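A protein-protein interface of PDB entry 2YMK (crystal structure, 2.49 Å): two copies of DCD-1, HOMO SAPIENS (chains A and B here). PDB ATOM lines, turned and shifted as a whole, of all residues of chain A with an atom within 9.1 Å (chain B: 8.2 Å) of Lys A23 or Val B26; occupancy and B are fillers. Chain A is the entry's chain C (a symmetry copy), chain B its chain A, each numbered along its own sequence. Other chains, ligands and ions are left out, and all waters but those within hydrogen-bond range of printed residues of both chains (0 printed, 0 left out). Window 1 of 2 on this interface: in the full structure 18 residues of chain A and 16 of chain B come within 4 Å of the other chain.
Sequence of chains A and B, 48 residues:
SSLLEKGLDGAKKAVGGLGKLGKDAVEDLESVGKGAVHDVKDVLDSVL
Of chain B, only Lys B23 and Val B26 come within 4 Å of Lys A23.
Printed residues of chain A within 4 Å of Val B26: Gly A19 (3.4 Å), Gly A22 (3.8 Å), Lys A23 (3.7 Å) and Val A26 (3.9 Å).
Of chain B, only Val B26 (3.8 Å) comes within 4 Å of Gly A22.
Of the printed residues of chain A, Glu B30 touches Val A15 and Gly A19.
Of the printed residues of chain A, Gly B22 touches Val A26 (3.98 Å).
Printed residues of chain A within 4 Å of Lys B23: Lys A23 (3.8 Å), Val A26 (3.8 Å), Glu A27 (2.9 Å) and Glu A30 (3.1 Å).
Printed residues of chain B within 4 Å of Glu A27: Lys B23 (2.9 Å).
The nearest residue of chain A that does not touch Val B26 is Leu A18 (5.0 Å).
The nearest printed residue of chain A that does not touch Gly B33 is Gly A16 (7.6 Å).
Hydrophobic or aromatic side chains of chain B within 4 Å of the printed part of chain A: Val B26.
Along chain A the printed residues that touch a printed residue of chain B span positions 15 to 30.
Among the printed residues, 13 pairs touch across the chains.
Among the printed residues, Asp or Glu carboxylates within 4 Å of a Lys or Arg side-chain nitrogen of the other chain: Glu A27 with Lys B23 (2.9 Å) and Glu A30 with Lys B23 (3.1 Å).
Gly A19 touches Val B26, and with the chains exchanged Val A26 touches Gly B19.
Gly A22 touches Val B26, and with the chains exchanged Val A26 touches Gly B22.
Lys A23 touches its own counterpart, Lys B23.
Lys A23 touches Val B26, and with the chains exchanged Val A26 touches Lys B23.
Positions printed for both chains: 19, 20, 21, 22, 23, 24, 25, 26, 27, 28, 29 and 30.
Of the 13 pairs that touch across the chains among the printed residues, 8 have their exchanged pair printed and touching as well.
Gly B33 touches Val A15 (CA to CG1, 3.95 Å).
Gly A19 touches Val B26.
Gly A19 touches Glu B30.
Gly A22 touches Val B26.
Lys A23 touches Lys B23 (CG to CG, 3.8 Å).
N of Lys A23 touches CG2 of Val B26, 3.7 Å away.
Gly B19 touches Val A26 (O to CG1, 3.7 Å).
Gly B22 touches Val A26.
Val A26 touches Lys B23 (CG1 to N, 3.8 Å).
Val B26 touches Val A26.
The side-chain amino group of Lys B23 is in salt-bridge range of the side-chain carboxylate of Glu A30 (3.1 Å).
The side-chain amino group (NZ) of Lys B23 is in salt-bridge range of the side-chain carboxylate (OE2) of Glu A27, at 2.9 Å.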
ATOM      1  N   VAL A  15      17.112 -30.362 -28.622  1.00  0.00           N
ATOM      2  CA  VAL A  15      17.402 -29.107 -27.938  1.00  0.00           C
ATOM      3  C   VAL A  15      18.850 -29.016 -27.521  1.00  0.00           C
ATOM      4  O   VAL A  15      19.429 -27.943 -27.509  1.00  0.00           O
ATOM      5  CB  VAL A  15      16.578 -28.935 -26.695  1.00  0.00           C
ATOM      6  CG1 VAL A  15      16.930 -27.642 -26.035  1.00  0.00           C
ATOM      7  CG2 VAL A  15      15.150 -28.920 -27.042  1.00  0.00           C
ATOM      8  N   GLY A  16      19.421 -30.153 -27.160  1.00  0.00           N
ATOM      9  CA  GLY A  16      20.777 -30.173 -26.646  1.00  0.00           C
ATOM     10  C   GLY A  16      21.723 -30.148 -27.834  1.00  0.00           C
ATOM     11  O   GLY A  16      22.784 -29.555 -27.781  1.00  0.00           O
ATOM     12  N   GLY A  17      21.333 -30.793 -28.923  1.00  0.00           N
ATOM     13  CA  GLY A  17      22.155 -30.843 -30.124  1.00  0.00           C
ATOM     14  C   GLY A  17      22.372 -29.442 -30.581  1.00  0.00           C
ATOM     15  O   GLY A  17      23.479 -28.979 -30.595  1.00  0.00           O
ATOM     16  N   LEU A  18      21.303 -28.734 -30.909  1.00  0.00           N
ATOM     17  CA  LEU A  18      21.404 -27.326 -31.298  1.00  0.00           C
ATOM     18  C   LEU A  18      22.195 -26.573 -30.278  1.00  0.00           C
ATOM     19  O   LEU A  18      22.911 -25.686 -30.620  1.00  0.00           O
ATOM     20  CB  LEU A  18      20.040 -26.665 -31.407  1.00  0.00           C
ATOM     21  CG  LEU A  18      19.009 -27.167 -32.421  1.00  0.00           C
ATOM     22  CD1 LEU A  18      17.639 -26.775 -31.909  1.00  0.00           C
ATOM     23  CD2 LEU A  18      19.220 -26.642 -33.847  1.00  0.00           C
ATOM     24  N   GLY A  19      22.085 -26.915 -29.017  1.00  0.00           N
ATOM     25  CA  GLY A  19      22.739 -26.111 -28.009  1.00  0.00           C
ATOM     26  C   GLY A  19      24.234 -26.293 -27.970  1.00  0.00           C
ATOM     27  O   GLY A  19      24.912 -25.571 -27.255  1.00  0.00           O
ATOM     28  N   LYS A  20      24.748 -27.275 -28.705  1.00  0.00           N
ATOM     29  CA  LYS A  20      26.194 -27.450 -28.871  1.00  0.00           C
ATOM     30  C   LYS A  20      26.669 -26.798 -30.147  1.00  0.00           C
ATOM     31  O   LYS A  20      27.657 -26.102 -30.149  1.00  0.00           O
ATOM     32  CB  LYS A  20      26.596 -28.932 -28.861  1.00  0.00           C
ATOM     33  CG  LYS A  20      28.122 -29.193 -28.995  1.00  0.00           C
ATOM     34  CD  LYS A  20      28.977 -28.282 -28.065  1.00  0.00           C
ATOM     35  CE  LYS A  20      30.429 -28.615 -28.258  1.00  0.00           C
ATOM     36  NZ  LYS A  20      30.395 -29.941 -28.967  1.00  0.00           N
ATOM     37  N   LEU A  21      25.975 -27.028 -31.242  1.00  0.00           N
ATOM     38  CA  LEU A  21      26.167 -26.222 -32.427  1.00  0.00           C
ATOM     39  C   LEU A  21      26.242 -24.765 -32.063  1.00  0.00           C
ATOM     40  O   LEU A  21      27.176 -24.107 -32.405  1.00  0.00           O
ATOM     41  CB  LEU A  21      25.002 -26.427 -33.382  1.00  0.00           C
ATOM     42  N   GLY A  22      25.250 -24.252 -31.378  1.00  0.00           N
ATOM     43  CA  GLY A  22      25.299 -22.921 -30.861  1.00  0.00           C
ATOM     44  C   GLY A  22      26.579 -22.477 -30.174  1.00  0.00           C
ATOM     45  O   GLY A  22      27.322 -21.648 -30.728  1.00  0.00           O
ATOM     46  N   LYS A  23      26.787 -22.966 -28.946  1.00  0.00           N
ATOM     47  CA  LYS A  23      27.979 -22.792 -28.102  1.00  0.00           C
ATOM     48  C   LYS A  23      29.294 -23.038 -28.749  1.00  0.00           C
ATOM     49  O   LYS A  23      30.248 -22.486 -28.292  1.00  0.00           O
ATOM     50  CB  LYS A  23      27.903 -23.674 -26.860  1.00  0.00           C
ATOM     51  CG  LYS A  23      27.667 -22.842 -25.531  1.00  0.00           C
ATOM     52  CD  LYS A  23      27.143 -23.631 -24.303  1.00  0.00           C
ATOM     53  CE  LYS A  23      28.209 -24.557 -23.693  1.00  0.00           C
ATOM     54  NZ  LYS A  23      27.618 -25.782 -22.982  1.00  0.00           N
ATOM     55  N   ASP A  24      29.340 -23.849 -29.809  1.00  0.00           N
ATOM     56  CA  ASP A  24      30.531 -24.087 -30.696  1.00  0.00           C
ATOM     57  C   ASP A  24      30.736 -23.041 -31.851  1.00  0.00           C
ATOM     58  O   ASP A  24      31.851 -22.579 -32.095  1.00  0.00           O
ATOM     59  CB  ASP A  24      30.394 -25.485 -31.270  1.00  0.00           C
ATOM     60  CG  ASP A  24      31.449 -25.836 -32.285  1.00  0.00           C
ATOM     61  OD1 ASP A  24      32.616 -25.409 -32.123  1.00  0.00           O
ATOM     62  OD2 ASP A  24      31.116 -26.623 -33.229  1.00  0.00           O
ATOM     63  N   ALA A  25      29.673 -22.665 -32.553  1.00  0.00           N
ATOM     64  CA  ALA A  25      29.698 -21.448 -33.305  1.00  0.00           C
ATOM     65  C   ALA A  25      30.103 -20.309 -32.378  1.00  0.00           C
ATOM     66  O   ALA A  25      31.116 -19.705 -32.570  1.00  0.00           O
ATOM     67  CB  ALA A  25      28.373 -21.186 -33.881  1.00  0.00           C
ATOM     68  N   VAL A  26      29.352 -20.000 -31.343  1.00  0.00           N
ATOM     69  CA  VAL A  26      29.760 -18.845 -30.561  1.00  0.00           C
ATOM     70  C   VAL A  26      31.182 -18.858 -30.096  1.00  0.00           C
ATOM     71  O   VAL A  26      31.747 -17.810 -29.885  1.00  0.00           O
ATOM     72  CB  VAL A  26      29.001 -18.631 -29.281  1.00  0.00           C
ATOM     73  CG1 VAL A  26      29.687 -17.498 -28.535  1.00  0.00           C
ATOM     74  CG2 VAL A  26      27.516 -18.313 -29.521  1.00  0.00           C
ATOM     75  N   GLU A  27      31.772 -20.013 -29.862  1.00  0.00           N
ATOM     76  CA  GLU A  27      33.172 -20.037 -29.405  1.00  0.00           C
ATOM     77  C   GLU A  27      34.146 -20.007 -30.557  1.00  0.00           C
ATOM     78  O   GLU A  27      35.084 -19.235 -30.559  1.00  0.00           O
ATOM     79  CB  GLU A  27      33.463 -21.221 -28.536  1.00  0.00           C
ATOM     80  CG  GLU A  27      33.489 -20.876 -27.074  1.00  0.00           C
ATOM     81  CD  GLU A  27      33.708 -22.116 -26.202  1.00  0.00           C
ATOM     82  OE1 GLU A  27      33.606 -23.303 -26.694  1.00  0.00           O
ATOM     83  OE2 GLU A  27      33.977 -21.877 -24.997  1.00  0.00           O
ATOM     84  N   ASP A  28      33.934 -20.827 -31.556  1.00  0.00           N
ATOM     85  CA  ASP A  28      34.608 -20.540 -32.771  1.00  0.00           C
ATOM     86  C   ASP A  28      34.600 -19.024 -33.111  1.00  0.00           C
ATOM     87  O   ASP A  28      35.576 -18.547 -33.611  1.00  0.00           O
ATOM     88  CB  ASP A  28      34.071 -21.433 -33.888  1.00  0.00           C
ATOM     89  CG  ASP A  28      34.375 -22.936 -33.637  1.00  0.00           C
ATOM     90  OD1 ASP A  28      35.154 -23.241 -32.670  1.00  0.00           O
ATOM     91  OD2 ASP A  28      33.835 -23.800 -34.409  1.00  0.00           O
ATOM     92  N   LEU A  29      33.572 -18.253 -32.770  1.00  0.00           N
ATOM     93  CA  LEU A  29      33.576 -16.806 -33.054  1.00  0.00           C
ATOM     94  C   LEU A  29      34.511 -16.037 -32.178  1.00  0.00           C
ATOM     95  O   LEU A  29      35.180 -15.141 -32.666  1.00  0.00           O
ATOM     96  CB  LEU A  29      32.195 -16.193 -32.904  1.00  0.00           C
ATOM     97  CG  LEU A  29      31.552 -16.114 -34.270  1.00  0.00           C
ATOM     98  CD1 LEU A  29      30.093 -15.726 -34.160  1.00  0.00           C
ATOM     99  CD2 LEU A  29      32.357 -15.138 -35.030  1.00  0.00           C
ATOM    100  N   GLU A  30      34.556 -16.376 -30.890  1.00  0.00           N
ATOM    101  CA  GLU A  30      35.361 -15.648 -29.968  1.00  0.00           C
ATOM    102  C   GLU A  30      36.781 -15.834 -30.418  1.00  0.00           C
ATOM    103  O   GLU A  30      37.607 -14.955 -30.278  1.00  0.00           O
ATOM    104  CB  GLU A  30      35.142 -16.232 -28.560  1.00  0.00           C
ATOM    105  CG  GLU A  30      35.774 -15.517 -27.286  1.00  0.00           C
ATOM    106  CD  GLU A  30      35.306 -16.196 -25.995  1.00  0.00           C
ATOM    107  OE1 GLU A  30      34.329 -16.937 -26.114  1.00  0.00           O
ATOM    108  OE2 GLU A  30      35.849 -16.029 -24.865  1.00  0.00           O
ATOM    109  N   GLY B  19      31.404 -12.564 -26.845  1.00  0.00           N
ATOM    110  CA  GLY B  19      31.405 -14.038 -26.703  1.00  0.00           C
ATOM    111  C   GLY B  19      30.759 -14.480 -25.411  1.00  0.00           C
ATOM    112  O   GLY B  19      30.011 -15.447 -25.413  1.00  0.00           O
ATOM    113  N   LYS B  20      31.021 -13.754 -24.320  1.00  0.00           N
ATOM    114  CA  LYS B  20      30.342 -13.964 -23.048  1.00  0.00           C
ATOM    115  C   LYS B  20      28.824 -13.760 -23.132  1.00  0.00           C
ATOM    116  O   LYS B  20      28.087 -14.598 -22.663  1.00  0.00           O
ATOM    117  CB  LYS B  20      30.946 -13.048 -21.972  1.00  0.00           C
ATOM    118  CG  LYS B  20      30.281 -13.130 -20.578  1.00  0.00           C
ATOM    119  CD  LYS B  20      30.041 -11.728 -20.018  1.00  0.00           C
ATOM    120  CE  LYS B  20      28.634 -11.652 -19.405  1.00  0.00           C
ATOM    121  NZ  LYS B  20      27.559 -12.049 -20.376  1.00  0.00           N
ATOM    122  N   LEU B  21      28.375 -12.649 -23.719  1.00  0.00           N
ATOM    123  CA  LEU B  21      26.971 -12.400 -24.035  1.00  0.00           C
ATOM    124  C   LEU B  21      26.323 -13.471 -24.910  1.00  0.00           C
ATOM    125  O   LEU B  21      25.183 -13.810 -24.720  1.00  0.00           O
ATOM    126  CB  LEU B  21      26.837 -11.060 -24.773  1.00  0.00           C
ATOM    127  CG  LEU B  21      25.585 -10.133 -24.568  1.00  0.00           C
ATOM    128  CD1 LEU B  21      24.981  -9.560 -25.896  1.00  0.00           C
ATOM    129  CD2 LEU B  21      24.415 -10.758 -23.658  1.00  0.00           C
ATOM    130  N   GLY B  22      27.043 -13.990 -25.882  1.00  0.00           N
ATOM    131  CA  GLY B  22      26.519 -15.013 -26.757  1.00  0.00           C
ATOM    132  C   GLY B  22      26.355 -16.423 -26.211  1.00  0.00           C
ATOM    133  O   GLY B  22      25.306 -17.007 -26.411  1.00  0.00           O
ATOM    134  N   LYS B  23      27.368 -17.006 -25.565  1.00  0.00           N
ATOM    135  CA  LYS B  23      27.234 -18.313 -24.887  1.00  0.00           C
ATOM    136  C   LYS B  23      26.210 -18.282 -23.768  1.00  0.00           C
ATOM    137  O   LYS B  23      25.667 -19.312 -23.426  1.00  0.00           O
ATOM    138  CB  LYS B  23      28.561 -18.768 -24.283  1.00  0.00           C
ATOM    139  CG  LYS B  23      29.513 -19.536 -25.263  1.00  0.00           C
ATOM    140  CD  LYS B  23      31.000 -19.028 -25.164  1.00  0.00           C
ATOM    141  CE  LYS B  23      31.932 -19.729 -24.117  1.00  0.00           C
ATOM    142  NZ  LYS B  23      33.356 -19.206 -24.217  1.00  0.00           N
ATOM    143  N   ASP B  24      25.930 -17.106 -23.200  1.00  0.00           N
ATOM    144  CA  ASP B  24      24.857 -16.892 -22.195  1.00  0.00           C
ATOM    145  C   ASP B  24      23.462 -16.742 -22.827  1.00  0.00           C
ATOM    146  O   ASP B  24      22.474 -16.685 -22.133  1.00  0.00           O
ATOM    147  CB  ASP B  24      25.218 -15.647 -21.448  1.00  0.00           C
ATOM    148  CG  ASP B  24      24.380 -15.397 -20.233  1.00  0.00           C
ATOM    149  OD1 ASP B  24      23.296 -15.992 -20.040  1.00  0.00           O
ATOM    150  OD2 ASP B  24      24.828 -14.532 -19.446  1.00  0.00           O
ATOM    151  N   ALA B  25      23.384 -16.666 -24.154  1.00  0.00           N
ATOM    152  CA  ALA B  25      22.140 -16.792 -24.870  1.00  0.00           C
ATOM    153  C   ALA B  25      21.961 -18.268 -25.187  1.00  0.00           C
ATOM    154  O   ALA B  25      20.951 -18.882 -24.852  1.00  0.00           O
ATOM    155  CB  ALA B  25      22.196 -16.019 -26.116  1.00  0.00           C
ATOM    156  N   VAL B  26      22.938 -18.872 -25.833  1.00  0.00           N
ATOM    157  CA  VAL B  26      22.797 -20.297 -26.102  1.00  0.00           C
ATOM    158  C   VAL B  26      22.355 -21.050 -24.841  1.00  0.00           C
ATOM    159  O   VAL B  26      21.429 -21.859 -24.909  1.00  0.00           O
ATOM    160  CB  VAL B  26      24.051 -20.946 -26.652  1.00  0.00           C
ATOM    161  CG1 VAL B  26      23.752 -22.400 -26.923  1.00  0.00           C
ATOM    162  CG2 VAL B  26      24.521 -20.238 -27.946  1.00  0.00           C
ATOM    163  N   GLU B  27      22.977 -20.752 -23.695  1.00  0.00           N
ATOM    164  CA  GLU B  27      22.692 -21.476 -22.461  1.00  0.00           C
ATOM    165  C   GLU B  27      21.296 -21.233 -21.929  1.00  0.00           C
ATOM    166  O   GLU B  27      20.727 -22.113 -21.278  1.00  0.00           O
ATOM    167  CB  GLU B  27      23.716 -21.171 -21.376  1.00  0.00           C
ATOM    168  CG  GLU B  27      24.726 -22.315 -21.126  1.00  0.00           C
ATOM    169  CD  GLU B  27      25.862 -21.912 -20.155  1.00  0.00           C
ATOM    170  OE1 GLU B  27      25.830 -20.758 -19.626  1.00  0.00           O
ATOM    171  OE2 GLU B  27      26.776 -22.756 -19.918  1.00  0.00           O
ATOM    172  N   ASP B  28      20.760 -20.043 -22.192  1.00  0.00           N
ATOM    173  CA  ASP B  28      19.416 -19.732 -21.789  1.00  0.00           C
ATOM    174  C   ASP B  28      18.403 -20.238 -22.785  1.00  0.00           C
ATOM    175  O   ASP B  28      17.313 -20.514 -22.429  1.00  0.00           O
ATOM    176  CB  ASP B  28      19.256 -18.262 -21.568  1.00  0.00           C
ATOM    177  CG  ASP B  28      19.908 -17.797 -20.292  1.00  0.00           C
ATOM    178  OD1 ASP B  28      20.037 -18.595 -19.319  1.00  0.00           O
ATOM    179  OD2 ASP B  28      20.301 -16.597 -20.263  1.00  0.00           O
ATOM    180  N   LEU B  29      18.755 -20.404 -24.035  1.00  0.00           N
ATOM    181  CA  LEU B  29      17.867 -21.075 -24.941  1.00  0.00           C
ATOM    182  C   LEU B  29      17.823 -22.570 -24.757  1.00  0.00           C
ATOM    183  O   LEU B  29      16.763 -23.103 -24.787  1.00  0.00           O
ATOM    184  CB  LEU B  29      18.251 -20.758 -26.356  1.00  0.00           C
ATOM    185  CG  LEU B  29      17.712 -19.414 -26.814  1.00  0.00           C
ATOM    186  CD1 LEU B  29      18.167 -19.284 -28.204  1.00  0.00           C
ATOM    187  CD2 LEU B  29      16.244 -19.500 -26.712  1.00  0.00           C
ATOM    188  N   GLU B  30      18.924 -23.276 -24.550  1.00  0.00           N
ATOM    189  CA  GLU B  30      18.782 -24.751 -24.331  1.00  0.00           C
ATOM    190  C   GLU B  30      17.999 -25.084 -23.077  1.00  0.00           C
ATOM    191  O   GLU B  30      17.151 -25.962 -23.085  1.00  0.00           O
ATOM    192  CB  GLU B  30      20.099 -25.585 -24.491  1.00  0.00           C
ATOM    193  CG  GLU B  30      21.108 -25.521 -23.410  1.00  0.00           C
ATOM    194  CD  GLU B  30      22.330 -26.379 -23.653  1.00  0.00           C
ATOM    195  OE1 GLU B  30      22.235 -27.614 -23.601  1.00  0.00           O
ATOM    196  OE2 GLU B  30      23.436 -25.836 -23.833  1.00  0.00           O
ATOM    197  N   SER B  31      18.238 -24.301 -22.036  1.00  0.00           N
ATOM    198  CA  SER B  31      17.545 -24.364 -20.766  1.00  0.00           C
ATOM    199  C   SER B  31      16.055 -24.027 -20.812  1.00  0.00           C
ATOM    200  O   SER B  31      15.279 -24.634 -20.151  1.00  0.00           O
ATOM    201  CB  SER B  31      18.277 -23.440 -19.813  1.00  0.00           C
ATOM    202  OG  SER B  31      17.375 -22.773 -18.953  1.00  0.00           O
ATOM    203  N   VAL B  32      15.638 -23.033 -21.559  1.00  0.00           N
ATOM    204  CA  VAL B  32      14.243 -22.930 -22.004  1.00  0.00           C
ATOM    205  C   VAL B  32      13.697 -24.279 -22.631  1.00  0.00           C
ATOM    206  O   VAL B  32      13.015 -25.038 -21.963  1.00  0.00           O
ATOM    207  CB  VAL B  32      14.156 -21.744 -23.026  1.00  0.00           C
ATOM    208  CG1 VAL B  32      12.821 -21.720 -23.773  1.00  0.00           C
ATOM    209  CG2 VAL B  32      14.372 -20.460 -22.312  1.00  0.00           C
ATOM    210  N   GLY B  33      13.999 -24.558 -23.905  1.00  0.00           N
ATOM    211  CA  GLY B  33      13.741 -25.860 -24.520  1.00  0.00           C
ATOM    212  C   GLY B  33      13.610 -26.991 -23.521  1.00  0.00           C
ATOM    213  O   GLY B  33      12.545 -27.529 -23.347  1.00  0.00           O
